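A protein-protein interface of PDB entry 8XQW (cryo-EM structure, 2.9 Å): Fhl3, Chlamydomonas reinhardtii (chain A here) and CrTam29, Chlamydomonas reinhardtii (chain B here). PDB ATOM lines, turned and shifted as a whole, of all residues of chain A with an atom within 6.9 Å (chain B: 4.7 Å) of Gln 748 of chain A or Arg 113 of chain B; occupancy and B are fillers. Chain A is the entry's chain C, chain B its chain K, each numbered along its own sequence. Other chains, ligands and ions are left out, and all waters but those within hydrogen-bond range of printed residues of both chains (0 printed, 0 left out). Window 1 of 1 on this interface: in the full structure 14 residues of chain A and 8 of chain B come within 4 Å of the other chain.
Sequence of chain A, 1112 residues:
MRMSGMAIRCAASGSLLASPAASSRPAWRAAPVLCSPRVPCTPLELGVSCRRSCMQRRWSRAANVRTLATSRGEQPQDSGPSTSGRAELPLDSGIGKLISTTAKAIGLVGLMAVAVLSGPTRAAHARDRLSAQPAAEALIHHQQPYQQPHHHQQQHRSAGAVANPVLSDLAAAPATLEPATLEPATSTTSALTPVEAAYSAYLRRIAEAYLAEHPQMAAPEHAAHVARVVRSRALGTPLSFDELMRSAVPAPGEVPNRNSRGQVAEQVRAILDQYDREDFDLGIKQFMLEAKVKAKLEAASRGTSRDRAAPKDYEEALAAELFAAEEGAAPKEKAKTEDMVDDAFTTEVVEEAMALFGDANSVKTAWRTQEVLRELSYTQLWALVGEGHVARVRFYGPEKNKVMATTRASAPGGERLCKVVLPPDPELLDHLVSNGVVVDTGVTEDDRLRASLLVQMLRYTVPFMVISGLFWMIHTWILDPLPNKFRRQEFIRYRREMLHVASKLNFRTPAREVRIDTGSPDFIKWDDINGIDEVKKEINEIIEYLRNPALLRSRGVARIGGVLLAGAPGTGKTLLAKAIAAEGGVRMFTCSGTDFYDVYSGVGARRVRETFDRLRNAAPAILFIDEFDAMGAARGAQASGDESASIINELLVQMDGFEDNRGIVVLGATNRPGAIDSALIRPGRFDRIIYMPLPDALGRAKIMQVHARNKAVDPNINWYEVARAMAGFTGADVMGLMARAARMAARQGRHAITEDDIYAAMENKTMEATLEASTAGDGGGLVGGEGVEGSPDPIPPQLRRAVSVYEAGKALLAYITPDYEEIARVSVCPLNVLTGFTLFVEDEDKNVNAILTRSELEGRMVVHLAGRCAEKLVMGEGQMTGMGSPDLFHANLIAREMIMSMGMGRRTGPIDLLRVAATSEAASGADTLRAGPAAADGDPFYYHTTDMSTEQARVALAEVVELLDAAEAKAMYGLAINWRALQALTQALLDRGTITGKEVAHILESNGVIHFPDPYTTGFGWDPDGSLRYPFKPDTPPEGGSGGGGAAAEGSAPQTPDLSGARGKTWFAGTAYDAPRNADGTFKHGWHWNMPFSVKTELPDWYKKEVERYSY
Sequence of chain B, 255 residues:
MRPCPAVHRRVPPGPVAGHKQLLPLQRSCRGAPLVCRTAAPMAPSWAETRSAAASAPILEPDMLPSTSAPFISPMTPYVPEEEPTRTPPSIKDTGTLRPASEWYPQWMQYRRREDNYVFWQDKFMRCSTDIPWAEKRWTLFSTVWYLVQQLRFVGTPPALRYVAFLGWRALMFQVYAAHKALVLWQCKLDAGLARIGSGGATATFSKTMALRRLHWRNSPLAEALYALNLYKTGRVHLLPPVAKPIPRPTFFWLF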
ATOM      1  N   ARG A 743      17.340   3.804  20.094  1.00  0.00           N
ATOM      2  CA  ARG A 743      17.945   2.534  20.507  1.00  0.00           C
ATOM      3  C   ARG A 743      17.488   1.378  19.620  1.00  0.00           C
ATOM      4  O   ARG A 743      18.292   0.521  19.218  1.00  0.00           O
ATOM      5  CB  ARG A 743      17.597   2.251  21.959  1.00  0.00           C
ATOM      6  CG  ARG A 743      18.760   1.824  22.793  1.00  0.00           C
ATOM      7  CD  ARG A 743      18.301   1.548  24.201  1.00  0.00           C
ATOM      8  NE  ARG A 743      17.683   2.724  24.796  1.00  0.00           N
ATOM      9  CZ  ARG A 743      16.683   2.680  25.667  1.00  0.00           C
ATOM     10  NH1 ARG A 743      16.181   1.515  26.044  1.00  0.00           N
ATOM     11  NH2 ARG A 743      16.183   3.801  26.160  1.00  0.00           N
ATOM     12  N   MET A 744      16.199   1.336  19.308  1.00  0.00           N
ATOM     13  CA  MET A 744      15.661   0.262  18.487  1.00  0.00           C
ATOM     14  C   MET A 744      16.151   0.345  17.053  1.00  0.00           C
ATOM     15  O   MET A 744      16.155  -0.660  16.344  1.00  0.00           O
ATOM     16  CB  MET A 744      14.138   0.304  18.530  1.00  0.00           C
ATOM     17  CG  MET A 744      13.480  -1.026  18.755  1.00  0.00           C
ATOM     18  SD  MET A 744      14.028  -1.850  20.247  1.00  0.00           S
ATOM     19  CE  MET A 744      13.745  -0.555  21.430  1.00  0.00           C
ATOM     20  N   ALA A 745      16.540   1.530  16.597  1.00  0.00           N
ATOM     21  CA  ALA A 745      17.121   1.661  15.267  1.00  0.00           C
ATOM     22  C   ALA A 745      18.570   1.227  15.262  1.00  0.00           C
ATOM     23  O   ALA A 745      19.060   0.702  14.263  1.00  0.00           O
ATOM     24  CB  ALA A 745      17.016   3.099  14.783  1.00  0.00           C
ATOM     25  N   ALA A 746      19.275   1.468  16.361  1.00  0.00           N
ATOM     26  CA  ALA A 746      20.618   0.920  16.486  1.00  0.00           C
ATOM     27  C   ALA A 746      20.593  -0.593  16.403  1.00  0.00           C
ATOM     28  O   ALA A 746      21.393  -1.195  15.687  1.00  0.00           O
ATOM     29  CB  ALA A 746      21.250   1.366  17.796  1.00  0.00           C
ATOM     30  N   ARG A 747      19.667  -1.226  17.112  1.00  0.00           N
ATOM     31  CA  ARG A 747      19.646  -2.688  17.132  1.00  0.00           C
ATOM     32  C   ARG A 747      19.368  -3.327  15.788  1.00  0.00           C
ATOM     33  O   ARG A 747      19.402  -4.552  15.714  1.00  0.00           O
ATOM     34  CB  ARG A 747      18.608  -3.195  18.116  1.00  0.00           C
ATOM     35  CG  ARG A 747      19.177  -3.531  19.437  1.00  0.00           C
ATOM     36  CD  ARG A 747      18.100  -3.940  20.376  1.00  0.00           C
ATOM     37  NE  ARG A 747      18.126  -3.114  21.568  1.00  0.00           N
ATOM     38  CZ  ARG A 747      17.308  -3.271  22.596  1.00  0.00           C
ATOM     39  NH1 ARG A 747      16.403  -4.234  22.572  1.00  0.00           N
ATOM     40  NH2 ARG A 747      17.396  -2.469  23.643  1.00  0.00           N
ATOM     41  N   GLN A 748      19.079  -2.575  14.734  1.00  0.00           N
ATOM     42  CA  GLN A 748      18.888  -3.166  13.417  1.00  0.00           C
ATOM     43  C   GLN A 748      19.941  -2.716  12.427  1.00  0.00           C
ATOM     44  O   GLN A 748      19.747  -2.873  11.223  1.00  0.00           O
ATOM     45  CB  GLN A 748      17.511  -2.838  12.861  1.00  0.00           C
ATOM     46  CG  GLN A 748      16.477  -3.883  13.148  1.00  0.00           C
ATOM     47  CD  GLN A 748      16.037  -4.633  11.926  1.00  0.00           C
ATOM     48  OE1 GLN A 748      15.435  -4.072  11.018  1.00  0.00           O
ATOM     49  NE2 GLN A 748      16.315  -5.920  11.903  1.00  0.00           N
ATOM     50  N   GLY A 749      21.036  -2.136  12.894  1.00  0.00           N
ATOM     51  CA  GLY A 749      22.047  -1.694  11.962  1.00  0.00           C
ATOM     52  C   GLY A 749      21.617  -0.527  11.111  1.00  0.00           C
ATOM     53  O   GLY A 749      21.834  -0.539   9.896  1.00  0.00           O
ATOM     54  N   ARG A 750      21.011   0.487  11.718  1.00  0.00           N
ATOM     55  CA  ARG A 750      20.635   1.697  11.011  1.00  0.00           C
ATOM     56  C   ARG A 750      20.971   2.905  11.864  1.00  0.00           C
ATOM     57  O   ARG A 750      21.233   2.793  13.059  1.00  0.00           O
ATOM     58  CB  ARG A 750      19.152   1.711  10.658  1.00  0.00           C
ATOM     59  CG  ARG A 750      18.785   0.714   9.600  1.00  0.00           C
ATOM     60  CD  ARG A 750      17.391   0.939   9.096  1.00  0.00           C
ATOM     61  NE  ARG A 750      16.461  -0.045   9.629  1.00  0.00           N
ATOM     62  CZ  ARG A 750      15.616   0.197  10.621  1.00  0.00           C
ATOM     63  NH1 ARG A 750      15.579   1.391  11.186  1.00  0.00           N
ATOM     64  NH2 ARG A 750      14.801  -0.753  11.046  1.00  0.00           N
ATOM     65  N   THR A 754      13.053   5.081  11.488  1.00  0.00           N
ATOM     66  CA  THR A 754      11.914   4.830  10.621  1.00  0.00           C
ATOM     67  C   THR A 754      10.660   4.684  11.468  1.00  0.00           C
ATOM     68  O   THR A 754      10.669   4.927  12.672  1.00  0.00           O
ATOM     69  CB  THR A 754      12.146   3.585   9.770  1.00  0.00           C
ATOM     70  OG1 THR A 754      12.982   2.671  10.482  1.00  0.00           O
ATOM     71  CG2 THR A 754      12.812   3.954   8.477  1.00  0.00           C
ATOM     72  N   ASP A 756       8.736   1.779  11.669  1.00  0.00           N
ATOM     73  CA  ASP A 756       8.685   0.489  12.331  1.00  0.00           C
ATOM     74  C   ASP A 756       9.585   0.478  13.550  1.00  0.00           C
ATOM     75  O   ASP A 756       9.388  -0.323  14.461  1.00  0.00           O
ATOM     76  CB  ASP A 756       9.059  -0.628  11.371  1.00  0.00           C
ATOM     77  CG  ASP A 756      10.392  -0.414  10.729  1.00  0.00           C
ATOM     78  OD1 ASP A 756      10.488   0.458   9.842  1.00  0.00           O
ATOM     79  OD2 ASP A 756      11.346  -1.127  11.101  1.00  0.00           O
ATOM     80  N   ASP A 757      10.547   1.393  13.611  1.00  0.00           N
ATOM     81  CA  ASP A 757      11.323   1.532  14.833  1.00  0.00           C
ATOM     82  C   ASP A 757      10.501   2.170  15.939  1.00  0.00           C
ATOM     83  O   ASP A 757      10.667   1.822  17.107  1.00  0.00           O
ATOM     84  CB  ASP A 757      12.584   2.326  14.551  1.00  0.00           C
ATOM     85  CG  ASP A 757      13.423   1.684  13.480  1.00  0.00           C
ATOM     86  OD1 ASP A 757      12.914   0.770  12.808  1.00  0.00           O
ATOM     87  OD2 ASP A 757      14.590   2.067  13.303  1.00  0.00           O
ATOM     88  N   ILE A 758       9.561   3.043  15.592  1.00  0.00           N
ATOM     89  CA  ILE A 758       8.660   3.586  16.600  1.00  0.00           C
ATOM     90  C   ILE A 758       7.695   2.514  17.091  1.00  0.00           C
ATOM     91  O   ILE A 758       7.465   2.366  18.302  1.00  0.00           O
ATOM     92  CB  ILE A 758       7.921   4.803  16.032  1.00  0.00           C
ATOM     93  CG1 ILE A 758       8.925   5.898  15.699  1.00  0.00           C
ATOM     94  CG2 ILE A 758       6.927   5.313  17.021  1.00  0.00           C
ATOM     95  CD1 ILE A 758       8.362   7.001  14.882  1.00  0.00           C
ATOM     96  N   ALA A 760       8.239  -0.680  17.062  1.00  0.00           N
ATOM     97  CA  ALA A 760       9.035  -1.603  17.847  1.00  0.00           C
ATOM     98  C   ALA A 760       9.349  -1.028  19.212  1.00  0.00           C
ATOM     99  O   ALA A 760       9.430  -1.765  20.193  1.00  0.00           O
ATOM    100  CB  ALA A 760      10.314  -1.947  17.101  1.00  0.00           C
ATOM    101  N   ALA A 761       9.516   0.288  19.307  1.00  0.00           N
ATOM    102  CA  ALA A 761       9.728   0.894  20.614  1.00  0.00           C
ATOM    103  C   ALA A 761       8.526   0.689  21.515  1.00  0.00           C
ATOM    104  O   ALA A 761       8.680   0.369  22.696  1.00  0.00           O
ATOM    105  CB  ALA A 761      10.020   2.378  20.467  1.00  0.00           C
ATOM    106  N   GLU A 763       6.164  -1.733  21.321  1.00  0.00           N
ATOM    107  CA  GLU A 763       6.115  -3.143  21.680  1.00  0.00           C
ATOM    108  C   GLU A 763       7.168  -3.490  22.721  1.00  0.00           C
ATOM    109  O   GLU A 763       6.907  -4.265  23.648  1.00  0.00           O
ATOM    110  CB  GLU A 763       6.291  -3.993  20.433  1.00  0.00           C
ATOM    111  CG  GLU A 763       7.093  -5.240  20.650  1.00  0.00           C
ATOM    112  CD  GLU A 763       7.599  -5.827  19.356  1.00  0.00           C
ATOM    113  OE1 GLU A 763       8.800  -5.659  19.055  1.00  0.00           O
ATOM    114  OE2 GLU A 763       6.792  -6.447  18.634  1.00  0.00           O
ATOM    115  N   ARG A 825       0.667  -4.144  14.339  1.00  0.00           N
ATOM    116  CA  ARG A 825       1.895  -4.920  14.303  1.00  0.00           C
ATOM    117  C   ARG A 825       1.648  -6.241  15.007  1.00  0.00           C
ATOM    118  O   ARG A 825       1.047  -6.258  16.078  1.00  0.00           O
ATOM    119  CB  ARG A 825       3.012  -4.141  14.984  1.00  0.00           C
ATOM    120  CG  ARG A 825       4.359  -4.771  14.935  1.00  0.00           C
ATOM    121  CD  ARG A 825       5.286  -4.028  15.860  1.00  0.00           C
ATOM    122  NE  ARG A 825       6.602  -4.639  15.917  1.00  0.00           N
ATOM    123  CZ  ARG A 825       7.556  -4.420  15.024  1.00  0.00           C
ATOM    124  NH1 ARG A 825       7.339  -3.602  14.005  1.00  0.00           N
ATOM    125  NH2 ARG A 825       8.727  -5.019  15.150  1.00  0.00           N
ATOM    126  N   THR A 994       7.795 -10.872  11.948  1.00  0.00           N
ATOM    127  CA  THR A 994       6.932  -9.760  12.306  1.00  0.00           C
ATOM    128  C   THR A 994       6.174  -9.299  11.075  1.00  0.00           C
ATOM    129  O   THR A 994       6.687  -9.335   9.959  1.00  0.00           O
ATOM    130  CB  THR A 994       7.741  -8.595  12.888  1.00  0.00           C
ATOM    131  OG1 THR A 994       8.597  -9.079  13.928  1.00  0.00           O
ATOM    132  CG2 THR A 994       6.830  -7.532  13.457  1.00  0.00           C
ATOM    133  N   MET B 108      22.886  -7.104   8.887  1.00  0.00           N
ATOM    134  CA  MET B 108      22.204  -6.831  10.143  1.00  0.00           C
ATOM    135  C   MET B 108      20.766  -6.397   9.932  1.00  0.00           C
ATOM    136  O   MET B 108      19.949  -6.507  10.846  1.00  0.00           O
ATOM    137  CB  MET B 108      22.950  -5.751  10.913  1.00  0.00           C
ATOM    138  CG  MET B 108      23.776  -6.250  12.047  1.00  0.00           C
ATOM    139  SD  MET B 108      24.582  -4.888  12.864  1.00  0.00           S
ATOM    140  CE  MET B 108      23.613  -4.760  14.340  1.00  0.00           C
ATOM    141  N   GLN B 109      20.438  -5.890   8.757  1.00  0.00           N
ATOM    142  CA  GLN B 109      19.101  -5.387   8.495  1.00  0.00           C
ATOM    143  C   GLN B 109      18.097  -6.475   8.185  1.00  0.00           C
ATOM    144  O   GLN B 109      16.907  -6.175   8.095  1.00  0.00           O
ATOM    145  CB  GLN B 109      19.128  -4.412   7.329  1.00  0.00           C
ATOM    146  CG  GLN B 109      19.942  -3.196   7.582  1.00  0.00           C
ATOM    147  CD  GLN B 109      19.829  -2.209   6.465  1.00  0.00           C
ATOM    148  OE1 GLN B 109      19.153  -2.459   5.474  1.00  0.00           O
ATOM    149  NE2 GLN B 109      20.494  -1.078   6.609  1.00  0.00           N
ATOM    150  N   ARG B 111      17.503  -9.413  10.001  1.00  0.00           N
ATOM    151  CA  ARG B 111      17.501 -10.316  11.134  1.00  0.00           C
ATOM    152  C   ARG B 111      16.690  -9.708  12.265  1.00  0.00           C
ATOM    153  O   ARG B 111      16.398  -8.515  12.277  1.00  0.00           O
ATOM    154  CB  ARG B 111      18.917 -10.611  11.615  1.00  0.00           C
ATOM    155  CG  ARG B 111      19.676 -11.559  10.739  1.00  0.00           C
ATOM    156  CD  ARG B 111      21.148 -11.469  10.989  1.00  0.00           C
ATOM    157  NE  ARG B 111      21.495 -11.744  12.372  1.00  0.00           N
ATOM    158  CZ  ARG B 111      21.980 -12.901  12.797  1.00  0.00           C
ATOM    159  NH1 ARG B 111      22.165 -13.885  11.945  1.00  0.00           N
ATOM    160  NH2 ARG B 111      22.281 -13.073  14.069  1.00  0.00           N
ATOM    161  N   ARG B 112      16.328 -10.544  13.224  1.00  0.00           N
ATOM    162  CA  ARG B 112      15.532 -10.077  14.345  1.00  0.00           C
ATOM    163  C   ARG B 112      16.371  -9.207  15.261  1.00  0.00           C
ATOM    164  O   ARG B 112      17.524  -9.519  15.540  1.00  0.00           O
ATOM    165  CB  ARG B 112      14.992 -11.265  15.126  1.00  0.00           C
ATOM    166  CG  ARG B 112      13.891 -12.018  14.446  1.00  0.00           C
ATOM    167  CD  ARG B 112      13.193 -12.879  15.459  1.00  0.00           C
ATOM    168  NE  ARG B 112      14.152 -13.514  16.353  1.00  0.00           N
ATOM    169  CZ  ARG B 112      13.936 -13.736  17.644  1.00  0.00           C
ATOM    170  NH1 ARG B 112      12.793 -13.368  18.201  1.00  0.00           N
ATOM    171  NH2 ARG B 112      14.867 -14.321  18.380  1.00  0.00           N
ATOM    172  N   ARG B 113      15.776  -8.124  15.759  1.00  0.00           N
ATOM    173  CA  ARG B 113      16.487  -7.248  16.680  1.00  0.00           C
ATOM    174  C   ARG B 113      17.066  -8.022  17.850  1.00  0.00           C
ATOM    175  O   ARG B 113      18.098  -7.639  18.408  1.00  0.00           O
ATOM    176  CB  ARG B 113      15.553  -6.161  17.198  1.00  0.00           C
ATOM    177  CG  ARG B 113      15.297  -5.053  16.228  1.00  0.00           C
ATOM    178  CD  ARG B 113      14.217  -4.126  16.719  1.00  0.00           C
ATOM    179  NE  ARG B 113      14.028  -3.008  15.808  1.00  0.00           N
ATOM    180  CZ  ARG B 113      13.247  -3.051  14.742  1.00  0.00           C
ATOM    181  NH1 ARG B 113      13.132  -1.997  13.957  1.00  0.00           N
ATOM    182  NH2 ARG B 113      12.578  -4.151  14.458  1.00  0.00           N
ATOM    183  N   GLU B 114      16.421  -9.092  18.244  1.00  0.00           N
ATOM    184  CA  GLU B 114      16.936  -9.873  19.357  1.00  0.00           C
ATOM    185  C   GLU B 114      17.872 -10.932  18.920  1.00  0.00           C
ATOM    186  O   GLU B 114      18.185 -11.824  19.697  1.00  0.00           O
ATOM    187  CB  GLU B 114      15.780 -10.482  20.148  1.00  0.00           C
ATOM    188  CG  GLU B 114      14.529 -10.727  19.326  1.00  0.00           C
ATOM    189  CD  GLU B 114      13.551  -9.569  19.362  1.00  0.00           C
ATOM    190  OE1 GLU B 114      13.039  -9.181  18.293  1.00  0.00           O
ATOM    191  OE2 GLU B 114      13.294  -9.041  20.460  1.00  0.00           O
ATOM    192  N   ASP B 115      18.323 -10.845  17.673  1.00  0.00           N
ATOM    193  CA  ASP B 115      19.343 -11.726  17.133  1.00  0.00           C
ATOM    194  C   ASP B 115      20.615 -11.007  16.746  1.00  0.00           C
ATOM    195  O   ASP B 115      21.603 -11.671  16.444  1.00  0.00           O
ATOM    196  CB  ASP B 115      18.819 -12.455  15.895  1.00  0.00           C
ATOM    197  CG  ASP B 115      18.431 -13.872  16.185  1.00  0.00           C
ATOM    198  OD1 ASP B 115      18.723 -14.345  17.298  1.00  0.00           O
ATOM    199  OD2 ASP B 115      17.831 -14.514  15.302  1.00  0.00           O
ATOM    200  N   ASN B 116      20.609  -9.680  16.712  1.00  0.00           N
ATOM    201  CA  ASN B 116      21.755  -8.875  16.315  1.00  0.00           C
ATOM    202  C   ASN B 116      22.646  -8.552  17.482  1.00  0.00           C
ATOM    203  O   ASN B 116      23.413  -7.598  17.433  1.00  0.00           O
ATOM    204  CB  ASN B 116      21.277  -7.598  15.648  1.00  0.00           C
ATOM    205  CG  ASN B 116      20.720  -7.839  14.299  1.00  0.00           C
ATOM    206  OD1 ASN B 116      20.978  -8.866  13.696  1.00  0.00           O
ATOM    207  ND2 ASN B 116      19.947  -6.897  13.804  1.00  0.00           N
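Among the printed residues, merely in contact across the chains: Gln 748 of chain A with Met 108 of chain B, Gln 748 of chain A with Gln 109 of chain B, Gln 748 of chain A with Arg 113 of chain B, Gln 748 of chain A with Asn 116 of chain B, Gly 749 of chain A with Met 108 of chain B, Gly 749 of chain A with Gln 109 of chain B, Arg 750 of chain A with Gln 109 of chain B, Arg 750 of chain A with Arg 113 of chain B and Ala 760 of chain A with Arg 113 of chain B.
O of Arg 747 of chain A is in hydrogen-bond range of ND2 of Asn 116 of chain B, at 3.1 Å. The backbone carbonyl oxygen (O) of Met 744 of chain A sits at hydrogen-bond distance from the guanidinium group (NE) of Arg 113 of chain B (3.2 Å). O of Arg 111 of chain B is in hydrogen-bond range of NE2 of Gln 748 of chain A, at 2.6 Å. The side-chain carboxylate (OD2) of Asp 756 of chain A lies within salt-bridge range of the guanidinium group (NH1) of Arg 113 of chain B, at 3.5 Å. The side-chain carboxylate (OD1) of Asp 757 of chain A lies within salt-bridge range of the guanidinium group (NH1) of Arg 113 of chain B, at 3.0 Å.
Of the printed residues of chain B, Arg 747 of chain A touches Asn 116 (3.1 Å). Printed residues of chain B within 4 Å of Gln 748 of chain A: Met 108, Gln 109, Arg 111, Arg 113 and Asn 116. Of the printed residues of chain B, Gly 749 of chain A touches Met 108 (3.95 Å) and Gln 109 (3.6 Å). Arg 825 of chain A touches none of the printed residues of chain B. Thr 994 of chain A touches none of the printed residues of chain B. Of the printed residues of chain A, Arg 113 of chain B touches Met 744, Gln 748, Arg 750, Asp 756, Asp 757 and Ala 760.
OG1 of Thr 754 of chain A is in hydrogen-bond range of OD1 of Asp 756 of chain A (3.4 Å). OD1 of Asp 757 of chain A sits at hydrogen-bond distance from OG1 of Thr 754 of chain A, 3.0 Å away. O of Ala 745 of chain A is in hydrogen-bond range of N of Arg 750 of chain A, 3.2 Å away. The guanidinium group (NH2) of Arg 750 of chain A is in hydrogen-bond range of the side-chain amide oxygen (OE1) of Gln 748 of chain A, 3.4 Å away. NH1 of Arg 750 of chain A is in salt-bridge range of OD2 of Asp 757 of chain A (2.4 Å). The guanidinium group of Arg 750 of chain A lies within hydrogen-bond range of the side-chain hydroxyl of Thr 754 of chain A, at 3.0 Å.
Hydrophobic or aromatic side chains of chain B within 4 Å of the printed part of chain A: Met 108. Of the 17 printed residues of chain A, 8 touch a printed residue of chain B. Hydrophobic or aromatic side chains of chain A within 4 Å of the printed part of chain B: Met 744 and Ala 760. Among the printed residues, 14 pairs touch across the chains. Among the printed residues, Asp or Glu carboxylates within 4 Å of a Lys or Arg side-chain nitrogen of the other chain: Asp 756 of chain A with Arg 113 of chain B (3.5 Å) and Asp 757 of chain A with Arg 113 of chain B (3.0 Å).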
